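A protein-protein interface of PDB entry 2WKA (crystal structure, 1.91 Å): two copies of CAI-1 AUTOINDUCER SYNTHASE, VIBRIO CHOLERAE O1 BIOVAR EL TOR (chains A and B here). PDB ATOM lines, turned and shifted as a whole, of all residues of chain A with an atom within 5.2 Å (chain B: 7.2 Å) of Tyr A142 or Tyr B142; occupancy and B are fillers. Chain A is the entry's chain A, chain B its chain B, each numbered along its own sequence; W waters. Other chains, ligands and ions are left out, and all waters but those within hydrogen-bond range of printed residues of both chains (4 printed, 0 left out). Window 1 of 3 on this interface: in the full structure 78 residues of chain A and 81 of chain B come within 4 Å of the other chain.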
ATOM      1  N   TRP A 109      10.487 -19.231 -25.489  1.00  0.00           N
ATOM      2  CA  TRP A 109       9.305 -20.086 -25.339  1.00  0.00           C
ATOM      3  C   TRP A 109       9.633 -21.491 -25.883  1.00  0.00           C
ATOM      4  O   TRP A 109       9.470 -22.495 -25.188  1.00  0.00           O
ATOM      5  CB  TRP A 109       8.090 -19.486 -26.070  1.00  0.00           C
ATOM      6  CG  TRP A 109       6.875 -20.383 -26.035  1.00  0.00           C
ATOM      7  CD1 TRP A 109       6.675 -21.507 -26.777  1.00  0.00           C
ATOM      8  CD2 TRP A 109       5.732 -20.262 -25.172  1.00  0.00           C
ATOM      9  NE1 TRP A 109       5.477 -22.089 -26.443  1.00  0.00           N
ATOM     10  CE2 TRP A 109       4.870 -21.342 -25.470  1.00  0.00           C
ATOM     11  CE3 TRP A 109       5.345 -19.338 -24.198  1.00  0.00           C
ATOM     12  CZ2 TRP A 109       3.645 -21.526 -24.821  1.00  0.00           C
ATOM     13  CZ3 TRP A 109       4.124 -19.524 -23.550  1.00  0.00           C
ATOM     14  CH2 TRP A 109       3.292 -20.607 -23.867  1.00  0.00           C
ATOM     15  N   VAL A 113       9.783 -25.198 -23.925  1.00  0.00           N
ATOM     16  CA  VAL A 113       8.863 -26.248 -24.376  1.00  0.00           C
ATOM     17  C   VAL A 113       9.658 -27.423 -24.919  1.00  0.00           C
ATOM     18  O   VAL A 113       9.332 -28.584 -24.642  1.00  0.00           O
ATOM     19  CB  VAL A 113       7.884 -25.735 -25.478  1.00  0.00           C
ATOM     20  CG1 VAL A 113       7.094 -26.880 -26.069  1.00  0.00           C
ATOM     21  CG2 VAL A 113       6.938 -24.688 -24.893  1.00  0.00           C
ATOM     22  N   GLU A 138       3.375 -24.551 -19.555  1.00  0.00           N
ATOM     23  CA  GLU A 138       2.854 -25.149 -20.785  1.00  0.00           C
ATOM     24  C   GLU A 138       3.730 -26.299 -21.293  1.00  0.00           C
ATOM     25  O   GLU A 138       3.224 -27.340 -21.728  1.00  0.00           O
ATOM     26  CB  GLU A 138       2.687 -24.085 -21.870  1.00  0.00           C
ATOM     27  CG  GLU A 138       1.496 -23.154 -21.661  1.00  0.00           C
ATOM     28  CD  GLU A 138       0.157 -23.885 -21.714  1.00  0.00           C
ATOM     29  OE1 GLU A 138      -0.445 -23.943 -22.806  1.00  0.00           O
ATOM     30  OE2 GLU A 138      -0.285 -24.406 -20.661  1.00  0.00           O
ATOM     31  N   GLY A 139       5.042 -26.100 -21.277  1.00  0.00           N
ATOM     32  CA  GLY A 139       5.968 -27.170 -21.633  1.00  0.00           C
ATOM     33  C   GLY A 139       5.675 -28.453 -20.874  1.00  0.00           C
ATOM     34  O   GLY A 139       5.663 -29.547 -21.449  1.00  0.00           O
ATOM     35  N   ALA A 140       5.442 -28.325 -19.571  1.00  0.00           N
ATOM     36  CA  ALA A 140       5.146 -29.490 -18.743  1.00  0.00           C
ATOM     37  C   ALA A 140       3.813 -30.106 -19.164  1.00  0.00           C
ATOM     38  O   ALA A 140       3.680 -31.327 -19.256  1.00  0.00           O
ATOM     39  CB  ALA A 140       5.111 -29.099 -17.265  1.00  0.00           C
ATOM     40  N   ARG A 141       2.836 -29.250 -19.434  1.00  0.00           N
ATOM     41  CA  ARG A 141       1.496 -29.699 -19.806  1.00  0.00           C
ATOM     42  C   ARG A 141       1.464 -30.407 -21.157  1.00  0.00           C
ATOM     43  O   ARG A 141       0.786 -31.424 -21.305  1.00  0.00           O
ATOM     44  CB  ARG A 141       0.501 -28.532 -19.788  1.00  0.00           C
ATOM     45  CG  ARG A 141      -0.946 -28.969 -20.067  1.00  0.00           C
ATOM     46  CD  ARG A 141      -1.920 -27.803 -19.962  1.00  0.00           C
ATOM     47  NE  ARG A 141      -1.827 -26.842 -21.065  1.00  0.00           N
ATOM     48  CZ  ARG A 141      -2.517 -26.934 -22.200  1.00  0.00           C
ATOM     49  NH1 ARG A 141      -3.348 -27.951 -22.400  1.00  0.00           N
ATOM     50  NH2 ARG A 141      -2.384 -26.007 -23.135  1.00  0.00           N
ATOM     51  N   TYR A 142       2.206 -29.884 -22.131  1.00  0.00           N
ATOM     52  CA  TYR A 142       2.307 -30.517 -23.445  1.00  0.00           C
ATOM     53  C   TYR A 142       2.923 -31.905 -23.357  1.00  0.00           C
ATOM     54  O   TYR A 142       2.604 -32.792 -24.157  1.00  0.00           O
ATOM     55  CB  TYR A 142       3.140 -29.669 -24.418  1.00  0.00           C
ATOM     56  CG  TYR A 142       2.632 -28.252 -24.640  1.00  0.00           C
ATOM     57  CD1 TYR A 142       1.340 -27.877 -24.278  1.00  0.00           C
ATOM     58  CD2 TYR A 142       3.436 -27.302 -25.248  1.00  0.00           C
ATOM     59  CE1 TYR A 142       0.882 -26.568 -24.484  1.00  0.00           C
ATOM     60  CE2 TYR A 142       2.990 -26.014 -25.470  1.00  0.00           C
ATOM     61  CZ  TYR A 142       1.716 -25.646 -25.084  1.00  0.00           C
ATOM     62  OH  TYR A 142       1.305 -24.342 -25.311  1.00  0.00           O
ATOM     63  N   ALA A 143       3.823 -32.077 -22.391  1.00  0.00           N
ATOM     64  CA  ALA A 143       4.520 -33.344 -22.185  1.00  0.00           C
ATOM     65  C   ALA A 143       3.712 -34.299 -21.311  1.00  0.00           C
ATOM     66  O   ALA A 143       4.166 -35.407 -20.998  1.00  0.00           O
ATOM     67  CB  ALA A 143       5.869 -33.090 -21.547  1.00  0.00           C
ATOM     68  N   ASN A 144       2.527 -33.857 -20.904  1.00  0.00           N
ATOM     69  CA  ASN A 144       1.669 -34.644 -20.023  1.00  0.00           C
ATOM     70  C   ASN A 144       2.352 -35.045 -18.707  1.00  0.00           C
ATOM     71  O   ASN A 144       2.029 -36.081 -18.118  1.00  0.00           O
ATOM     72  CB  ASN A 144       1.112 -35.868 -20.763  1.00  0.00           C
ATOM     73  CG  ASN A 144       0.022 -35.502 -21.761  1.00  0.00           C
ATOM     74  OD1 ASN A 144       0.151 -35.746 -22.965  1.00  0.00           O
ATOM     75  ND2 ASN A 144      -1.057 -34.905 -21.266  1.00  0.00           N
ATOM     76  N   TRP B 109       4.219 -22.120 -37.386  1.00  0.00           N
ATOM     77  CA  TRP B 109       3.839 -22.931 -36.217  1.00  0.00           C
ATOM     78  C   TRP B 109       2.963 -22.120 -35.257  1.00  0.00           C
ATOM     79  O   TRP B 109       1.865 -22.558 -34.877  1.00  0.00           O
ATOM     80  CB  TRP B 109       5.083 -23.488 -35.483  1.00  0.00           C
ATOM     81  CG  TRP B 109       4.761 -24.219 -34.200  1.00  0.00           C
ATOM     82  CD1 TRP B 109       4.476 -23.662 -32.985  1.00  0.00           C
ATOM     83  CD2 TRP B 109       4.697 -25.644 -34.009  1.00  0.00           C
ATOM     84  NE1 TRP B 109       4.236 -24.644 -32.057  1.00  0.00           N
ATOM     85  CE2 TRP B 109       4.349 -25.869 -32.658  1.00  0.00           C
ATOM     86  CE3 TRP B 109       4.895 -26.748 -34.848  1.00  0.00           C
ATOM     87  CZ2 TRP B 109       4.208 -27.152 -32.121  1.00  0.00           C
ATOM     88  CZ3 TRP B 109       4.746 -28.027 -34.315  1.00  0.00           C
ATOM     89  CH2 TRP B 109       4.404 -28.214 -32.964  1.00  0.00           C
ATOM     90  N   VAL B 113      -1.076 -22.540 -34.174  1.00  0.00           N
ATOM     91  CA  VAL B 113      -1.332 -22.767 -32.758  1.00  0.00           C
ATOM     92  C   VAL B 113      -2.185 -21.646 -32.145  1.00  0.00           C
ATOM     93  O   VAL B 113      -3.132 -21.909 -31.381  1.00  0.00           O
ATOM     94  CB  VAL B 113      -0.010 -22.951 -31.986  1.00  0.00           C
ATOM     95  CG1 VAL B 113      -0.200 -22.668 -30.495  1.00  0.00           C
ATOM     96  CG2 VAL B 113       0.527 -24.378 -32.229  1.00  0.00           C
ATOM     97  N   GLN B 117      -6.043 -21.824 -30.840  1.00  0.00           N
ATOM     98  CA  GLN B 117      -6.309 -21.493 -29.449  1.00  0.00           C
ATOM     99  C   GLN B 117      -7.401 -20.437 -29.335  1.00  0.00           C
ATOM    100  O   GLN B 117      -8.180 -20.453 -28.395  1.00  0.00           O
ATOM    101  CB  GLN B 117      -5.050 -21.001 -28.733  1.00  0.00           C
ATOM    102  CG  GLN B 117      -5.342 -20.472 -27.340  1.00  0.00           C
ATOM    103  CD  GLN B 117      -4.083 -20.237 -26.534  1.00  0.00           C
ATOM    104  OE1 GLN B 117      -2.975 -20.156 -27.087  1.00  0.00           O
ATOM    105  NE2 GLN B 117      -4.239 -20.132 -25.219  1.00  0.00           N
ATOM    106  N   MET B 134       1.891 -30.839 -38.289  1.00  0.00           N
ATOM    107  CA  MET B 134       1.946 -31.131 -36.879  1.00  0.00           C
ATOM    108  C   MET B 134       1.499 -29.946 -36.020  1.00  0.00           C
ATOM    109  O   MET B 134       0.936 -30.141 -34.962  1.00  0.00           O
ATOM    110  CB  MET B 134       3.363 -31.601 -36.482  1.00  0.00           C
ATOM    111  CG  MET B 134       3.503 -31.991 -35.021  1.00  0.00           C
ATOM    112  SD  MET B 134       2.546 -33.461 -34.567  1.00  0.00           S
ATOM    113  CE  MET B 134       3.606 -34.746 -35.241  1.00  0.00           C
ATOM    114  N   SER B 135       1.751 -28.725 -36.476  1.00  0.00           N
ATOM    115  CA  SER B 135       1.352 -27.532 -35.725  1.00  0.00           C
ATOM    116  C   SER B 135      -0.173 -27.443 -35.550  1.00  0.00           C
ATOM    117  O   SER B 135      -0.654 -26.924 -34.548  1.00  0.00           O
ATOM    118  CB  SER B 135       1.846 -26.274 -36.426  1.00  0.00           C
ATOM    119  OG  SER B 135       1.461 -26.269 -37.790  1.00  0.00           O
ATOM    120  N   LEU B 136      -0.913 -27.908 -36.553  1.00  0.00           N
ATOM    121  CA  LEU B 136      -2.381 -27.921 -36.480  1.00  0.00           C
ATOM    122  C   LEU B 136      -2.844 -29.008 -35.518  1.00  0.00           C
ATOM    123  O   LEU B 136      -3.733 -28.783 -34.698  1.00  0.00           O
ATOM    124  CB  LEU B 136      -2.992 -28.099 -37.878  1.00  0.00           C
ATOM    125  CG  LEU B 136      -2.633 -26.998 -38.885  1.00  0.00           C
ATOM    126  CD1 LEU B 136      -2.768 -27.471 -40.325  1.00  0.00           C
ATOM    127  CD2 LEU B 136      -3.474 -25.750 -38.650  1.00  0.00           C
ATOM    128  N   TRP B 137      -2.225 -30.180 -35.602  1.00  0.00           N
ATOM    129  CA  TRP B 137      -2.499 -31.240 -34.638  1.00  0.00           C
ATOM    130  C   TRP B 137      -2.233 -30.771 -33.220  1.00  0.00           C
ATOM    131  O   TRP B 137      -3.065 -30.940 -32.328  1.00  0.00           O
ATOM    132  CB  TRP B 137      -1.643 -32.474 -34.934  1.00  0.00           C
ATOM    133  CG  TRP B 137      -2.131 -33.279 -36.095  1.00  0.00           C
ATOM    134  CD1 TRP B 137      -1.899 -33.044 -37.421  1.00  0.00           C
ATOM    135  CD2 TRP B 137      -2.937 -34.460 -36.030  1.00  0.00           C
ATOM    136  NE1 TRP B 137      -2.514 -34.011 -38.185  1.00  0.00           N
ATOM    137  CE2 TRP B 137      -3.151 -34.894 -37.352  1.00  0.00           C
ATOM    138  CE3 TRP B 137      -3.494 -35.195 -34.977  1.00  0.00           C
ATOM    139  CZ2 TRP B 137      -3.900 -36.032 -37.655  1.00  0.00           C
ATOM    140  CZ3 TRP B 137      -4.238 -36.332 -35.281  1.00  0.00           C
ATOM    141  CH2 TRP B 137      -4.429 -36.736 -36.611  1.00  0.00           C
ATOM    142  N   GLU B 138      -1.065 -30.180 -32.998  1.00  0.00           N
ATOM    143  CA  GLU B 138      -0.727 -29.718 -31.659  1.00  0.00           C
ATOM    144  C   GLU B 138      -1.570 -28.524 -31.199  1.00  0.00           C
ATOM    145  O   GLU B 138      -1.901 -28.410 -30.015  1.00  0.00           O
ATOM    146  CB  GLU B 138       0.769 -29.397 -31.561  1.00  0.00           C
ATOM    147  CG  GLU B 138       1.668 -30.639 -31.553  1.00  0.00           C
ATOM    148  CD  GLU B 138       1.482 -31.482 -30.298  1.00  0.00           C
ATOM    149  OE1 GLU B 138       2.282 -31.327 -29.350  1.00  0.00           O
ATOM    150  OE2 GLU B 138       0.526 -32.287 -30.249  1.00  0.00           O
ATOM    151  N   GLY B 139      -1.898 -27.626 -32.120  1.00  0.00           N
ATOM    152  CA  GLY B 139      -2.717 -26.474 -31.752  1.00  0.00           C
ATOM    153  C   GLY B 139      -4.068 -26.920 -31.205  1.00  0.00           C
ATOM    154  O   GLY B 139      -4.591 -26.328 -30.253  1.00  0.00           O
ATOM    155  N   ALA B 140      -4.639 -27.949 -31.820  1.00  0.00           N
ATOM    156  CA  ALA B 140      -5.940 -28.487 -31.380  1.00  0.00           C
ATOM    157  C   ALA B 140      -5.768 -29.141 -30.024  1.00  0.00           C
ATOM    158  O   ALA B 140      -6.555 -28.945 -29.090  1.00  0.00           O
ATOM    159  CB  ALA B 140      -6.469 -29.511 -32.394  1.00  0.00           C
ATOM    160  N   ARG B 141      -4.708 -29.923 -29.922  1.00  0.00           N
ATOM    161  CA  ARG B 141      -4.378 -30.618 -28.700  1.00  0.00           C
ATOM    162  C   ARG B 141      -4.174 -29.644 -27.517  1.00  0.00           C
ATOM    163  O   ARG B 141      -4.778 -29.812 -26.455  1.00  0.00           O
ATOM    164  CB  ARG B 141      -3.130 -31.451 -28.975  1.00  0.00           C
ATOM    165  CG  ARG B 141      -2.909 -32.610 -28.061  1.00  0.00           C
ATOM    166  CD  ARG B 141      -1.442 -32.966 -28.105  1.00  0.00           C
ATOM    167  NE  ARG B 141      -1.036 -33.259 -26.754  1.00  0.00           N
ATOM    168  CZ  ARG B 141       0.153 -33.019 -26.229  1.00  0.00           C
ATOM    169  NH1 ARG B 141       1.142 -32.460 -26.932  1.00  0.00           N
ATOM    170  NH2 ARG B 141       0.329 -33.361 -24.975  1.00  0.00           N
ATOM    171  N   TYR B 142      -3.347 -28.614 -27.688  1.00  0.00           N
ATOM    172  CA  TYR B 142      -3.141 -27.646 -26.604  1.00  0.00           C
ATOM    173  C   TYR B 142      -4.471 -27.024 -26.167  1.00  0.00           C
ATOM    174  O   TYR B 142      -4.644 -26.661 -25.005  1.00  0.00           O
ATOM    175  CB  TYR B 142      -2.202 -26.501 -27.024  1.00  0.00           C
ATOM    176  CG  TYR B 142      -0.825 -26.898 -27.514  1.00  0.00           C
ATOM    177  CD1 TYR B 142      -0.294 -28.152 -27.236  1.00  0.00           C
ATOM    178  CD2 TYR B 142      -0.042 -25.996 -28.226  1.00  0.00           C
ATOM    179  CE1 TYR B 142       0.967 -28.505 -27.685  1.00  0.00           C
ATOM    180  CE2 TYR B 142       1.217 -26.335 -28.667  1.00  0.00           C
ATOM    181  CZ  TYR B 142       1.712 -27.589 -28.396  1.00  0.00           C
ATOM    182  OH  TYR B 142       2.969 -27.925 -28.833  1.00  0.00           O
ATOM    183  N   ALA B 143      -5.384 -26.866 -27.117  1.00  0.00           N
ATOM    184  CA  ALA B 143      -6.697 -26.263 -26.852  1.00  0.00           C
ATOM    185  C   ALA B 143      -7.669 -27.274 -26.241  1.00  0.00           C
ATOM    186  O   ALA B 143      -8.836 -26.952 -25.963  1.00  0.00           O
ATOM    187  CB  ALA B 143      -7.273 -25.691 -28.133  1.00  0.00           C
ATOM    188  N   ASN B 144      -7.184 -28.495 -26.028  1.00  0.00           N
ATOM    189  CA  ASN B 144      -8.031 -29.591 -25.558  1.00  0.00           C
ATOM    190  C   ASN B 144      -9.274 -29.806 -26.429  1.00  0.00           C
ATOM    191  O   ASN B 144     -10.328 -30.237 -25.949  1.00  0.00           O
ATOM    192  CB  ASN B 144      -8.425 -29.372 -24.097  1.00  0.00           C
ATOM    193  CG  ASN B 144      -7.244 -29.504 -23.160  1.00  0.00           C
ATOM    194  OD1 ASN B 144      -6.924 -28.580 -22.426  1.00  0.00           O
ATOM    195  ND2 ASN B 144      -6.582 -30.653 -23.194  1.00  0.00           N
ATOM    196  N   ALA B 145      -9.138 -29.499 -27.711  1.00  0.00           N
ATOM    197  CA  ALA B 145     -10.221 -29.676 -28.662  1.00  0.00           C
ATOM    198  C   ALA B 145     -10.441 -31.165 -28.891  1.00  0.00           C
ATOM    199  O   ALA B 145      -9.598 -31.981 -28.517  1.00  0.00           O
ATOM    200  CB  ALA B 145      -9.881 -28.985 -29.959  1.00  0.00           C
ATOM    201  N   TYR B 260      -1.233 -17.942 -26.716  1.00  0.00           N
ATOM    202  CA  TYR B 260      -0.070 -17.925 -25.825  1.00  0.00           C
ATOM    203  C   TYR B 260       1.234 -17.505 -26.522  1.00  0.00           C
ATOM    204  O   TYR B 260       2.002 -16.721 -25.966  1.00  0.00           O
ATOM    205  CB  TYR B 260       0.073 -19.252 -25.080  1.00  0.00           C
ATOM    206  CG  TYR B 260      -0.859 -19.365 -23.887  1.00  0.00           C
ATOM    207  CD1 TYR B 260      -1.828 -18.396 -23.637  1.00  0.00           C
ATOM    208  CD2 TYR B 260      -0.767 -20.433 -23.012  1.00  0.00           C
ATOM    209  CE1 TYR B 260      -2.683 -18.495 -22.544  1.00  0.00           C
ATOM    210  CE2 TYR B 260      -1.608 -20.536 -21.910  1.00  0.00           C
ATOM    211  CZ  TYR B 260      -2.563 -19.569 -21.681  1.00  0.00           C
ATOM    212  OH  TYR B 260      -3.405 -19.679 -20.583  1.00  0.00           O
ATOM    213  N   PRO B 261       1.503 -18.043 -27.723  1.00  0.00           N
ATOM    214  CA  PRO B 261       2.673 -17.585 -28.487  1.00  0.00           C
ATOM    215  C   PRO B 261       2.607 -16.085 -28.804  1.00  0.00           C
ATOM    216  O   PRO B 261       3.626 -15.394 -28.763  1.00  0.00           O
ATOM    217  CB  PRO B 261       2.598 -18.425 -29.765  1.00  0.00           C
ATOM    218  CG  PRO B 261       1.975 -19.741 -29.269  1.00  0.00           C
ATOM    219  CD  PRO B 261       0.920 -19.277 -28.289  1.00  0.00           C
HETATM  220  O   HOH W   1      -5.319 -28.838 -20.351  1.00  0.00           O
HETATM  221  O   HOH W   2      -3.686 -30.717 -21.542  1.00  0.00           O
HETATM  222  O   HOH W   3      -2.591 -33.675 -24.092  1.00  0.00           O
HETATM  223  O   HOH W   4       2.975 -35.294 -25.243  1.00  0.00           O
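Among the printed residues, merely in contact across the chains: Trp A109 with Tyr B260 (3.7 Å), Glu A138 with Tyr B260 (3.5 Å), Arg A141 with Asn B144 (3.6 Å) and Tyr A142 with Tyr B142 (3.4 Å).
Printed residues of chain A that touch a printed residue of chain B: Trp A109, Glu A138, Arg A141, Tyr A142 and Asn A144.
Of the 17 printed residues of chain B, 4 touch a printed residue of chain A.
Hydrophobic or aromatic side chains of chain B that line the printed part of chain A: Tyr B142 and Tyr B260.
Among the printed residues, 7 pairs touch across the chains.
Among the printed residues, no Asp or Glu carboxylate lies within 4 Å of a Lys or Arg side-chain nitrogen of the other chain.
Of the printed residues of chain B, Trp A109 touches Tyr B260 (3.7 Å).
Of the printed residues of chain B, Glu A138 touches Tyr B260 (3.5 Å).
Of the printed residues of chain B, Arg A141 touches Tyr B142 and Asn B144.
Printed residues of chain B within 4 Å of Tyr A142: Arg B141 (2.5 Å) and Tyr B142 (3.4 Å).
Printed residues of chain B within 4 Å of Asn A144: Arg B141.
Trp B109 touches none of the printed residues of chain A.
Of the printed residues of chain A, Arg B141 touches Tyr A142 and Asn A144.
NH2 of Arg B141 is in hydrogen-bond range of O of Tyr A142 (2.5 Å).
OD1 of Asn A144 lies within hydrogen-bond range of NH2 of Arg B141, at 3.1 Å.
The guanidinium group of Arg A141 is in hydrogen-bond range of the backbone carbonyl oxygen of Tyr B142, at 3.0 Å.
Arg A141 touches Tyr B142, and with the chains exchanged Tyr A142 touches Arg B141.
Arg A141 touches Asn B144, and with the chains exchanged Asn A144 touches Arg B141.
Tyr A142 touches its own counterpart, Tyr B142.
9 positions are printed for both chains.
Of the 7 pairs that touch across the chains among the printed residues, 5 have their exchanged pair printed and touching as well.
OE1 of Glu A138 sits at hydrogen-bond distance from OH of Tyr A142 (3.1 Å).
OE1 of Glu B138 lies within salt-bridge range of NH1 of Arg B141 (2.9 Å).
The side-chain carboxylate of Glu A138 lies within salt-bridge range of the guanidinium group of Arg A141 (2.9 Å).
The side-chain amide oxygen (OE1) of Gln B117 sits at hydrogen-bond distance from the backbone NH (N) of Tyr B260 (2.8 Å).
Water W1 lies within hydrogen-bond range of the side-chain amide oxygen of Asn B144 (2.6 Å) and the guanidinium group of Arg A141 (3.0 Å).
Water W4 lies within hydrogen-bond range of the backbone carbonyl oxygen (O) of Tyr A142 (2.8 Å) and the guanidinium group (NH2) of Arg B141 (3.3 Å).
Water W2 bridges the guanidinium group of Arg A141 (2.9 Å) and the side-chain amide nitrogen of Asn B144 (3.3 Å).
Water W3 bridges NH2 of Arg B141 (3.1 Å) and ND2 of Asn A144 (3.4 Å).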
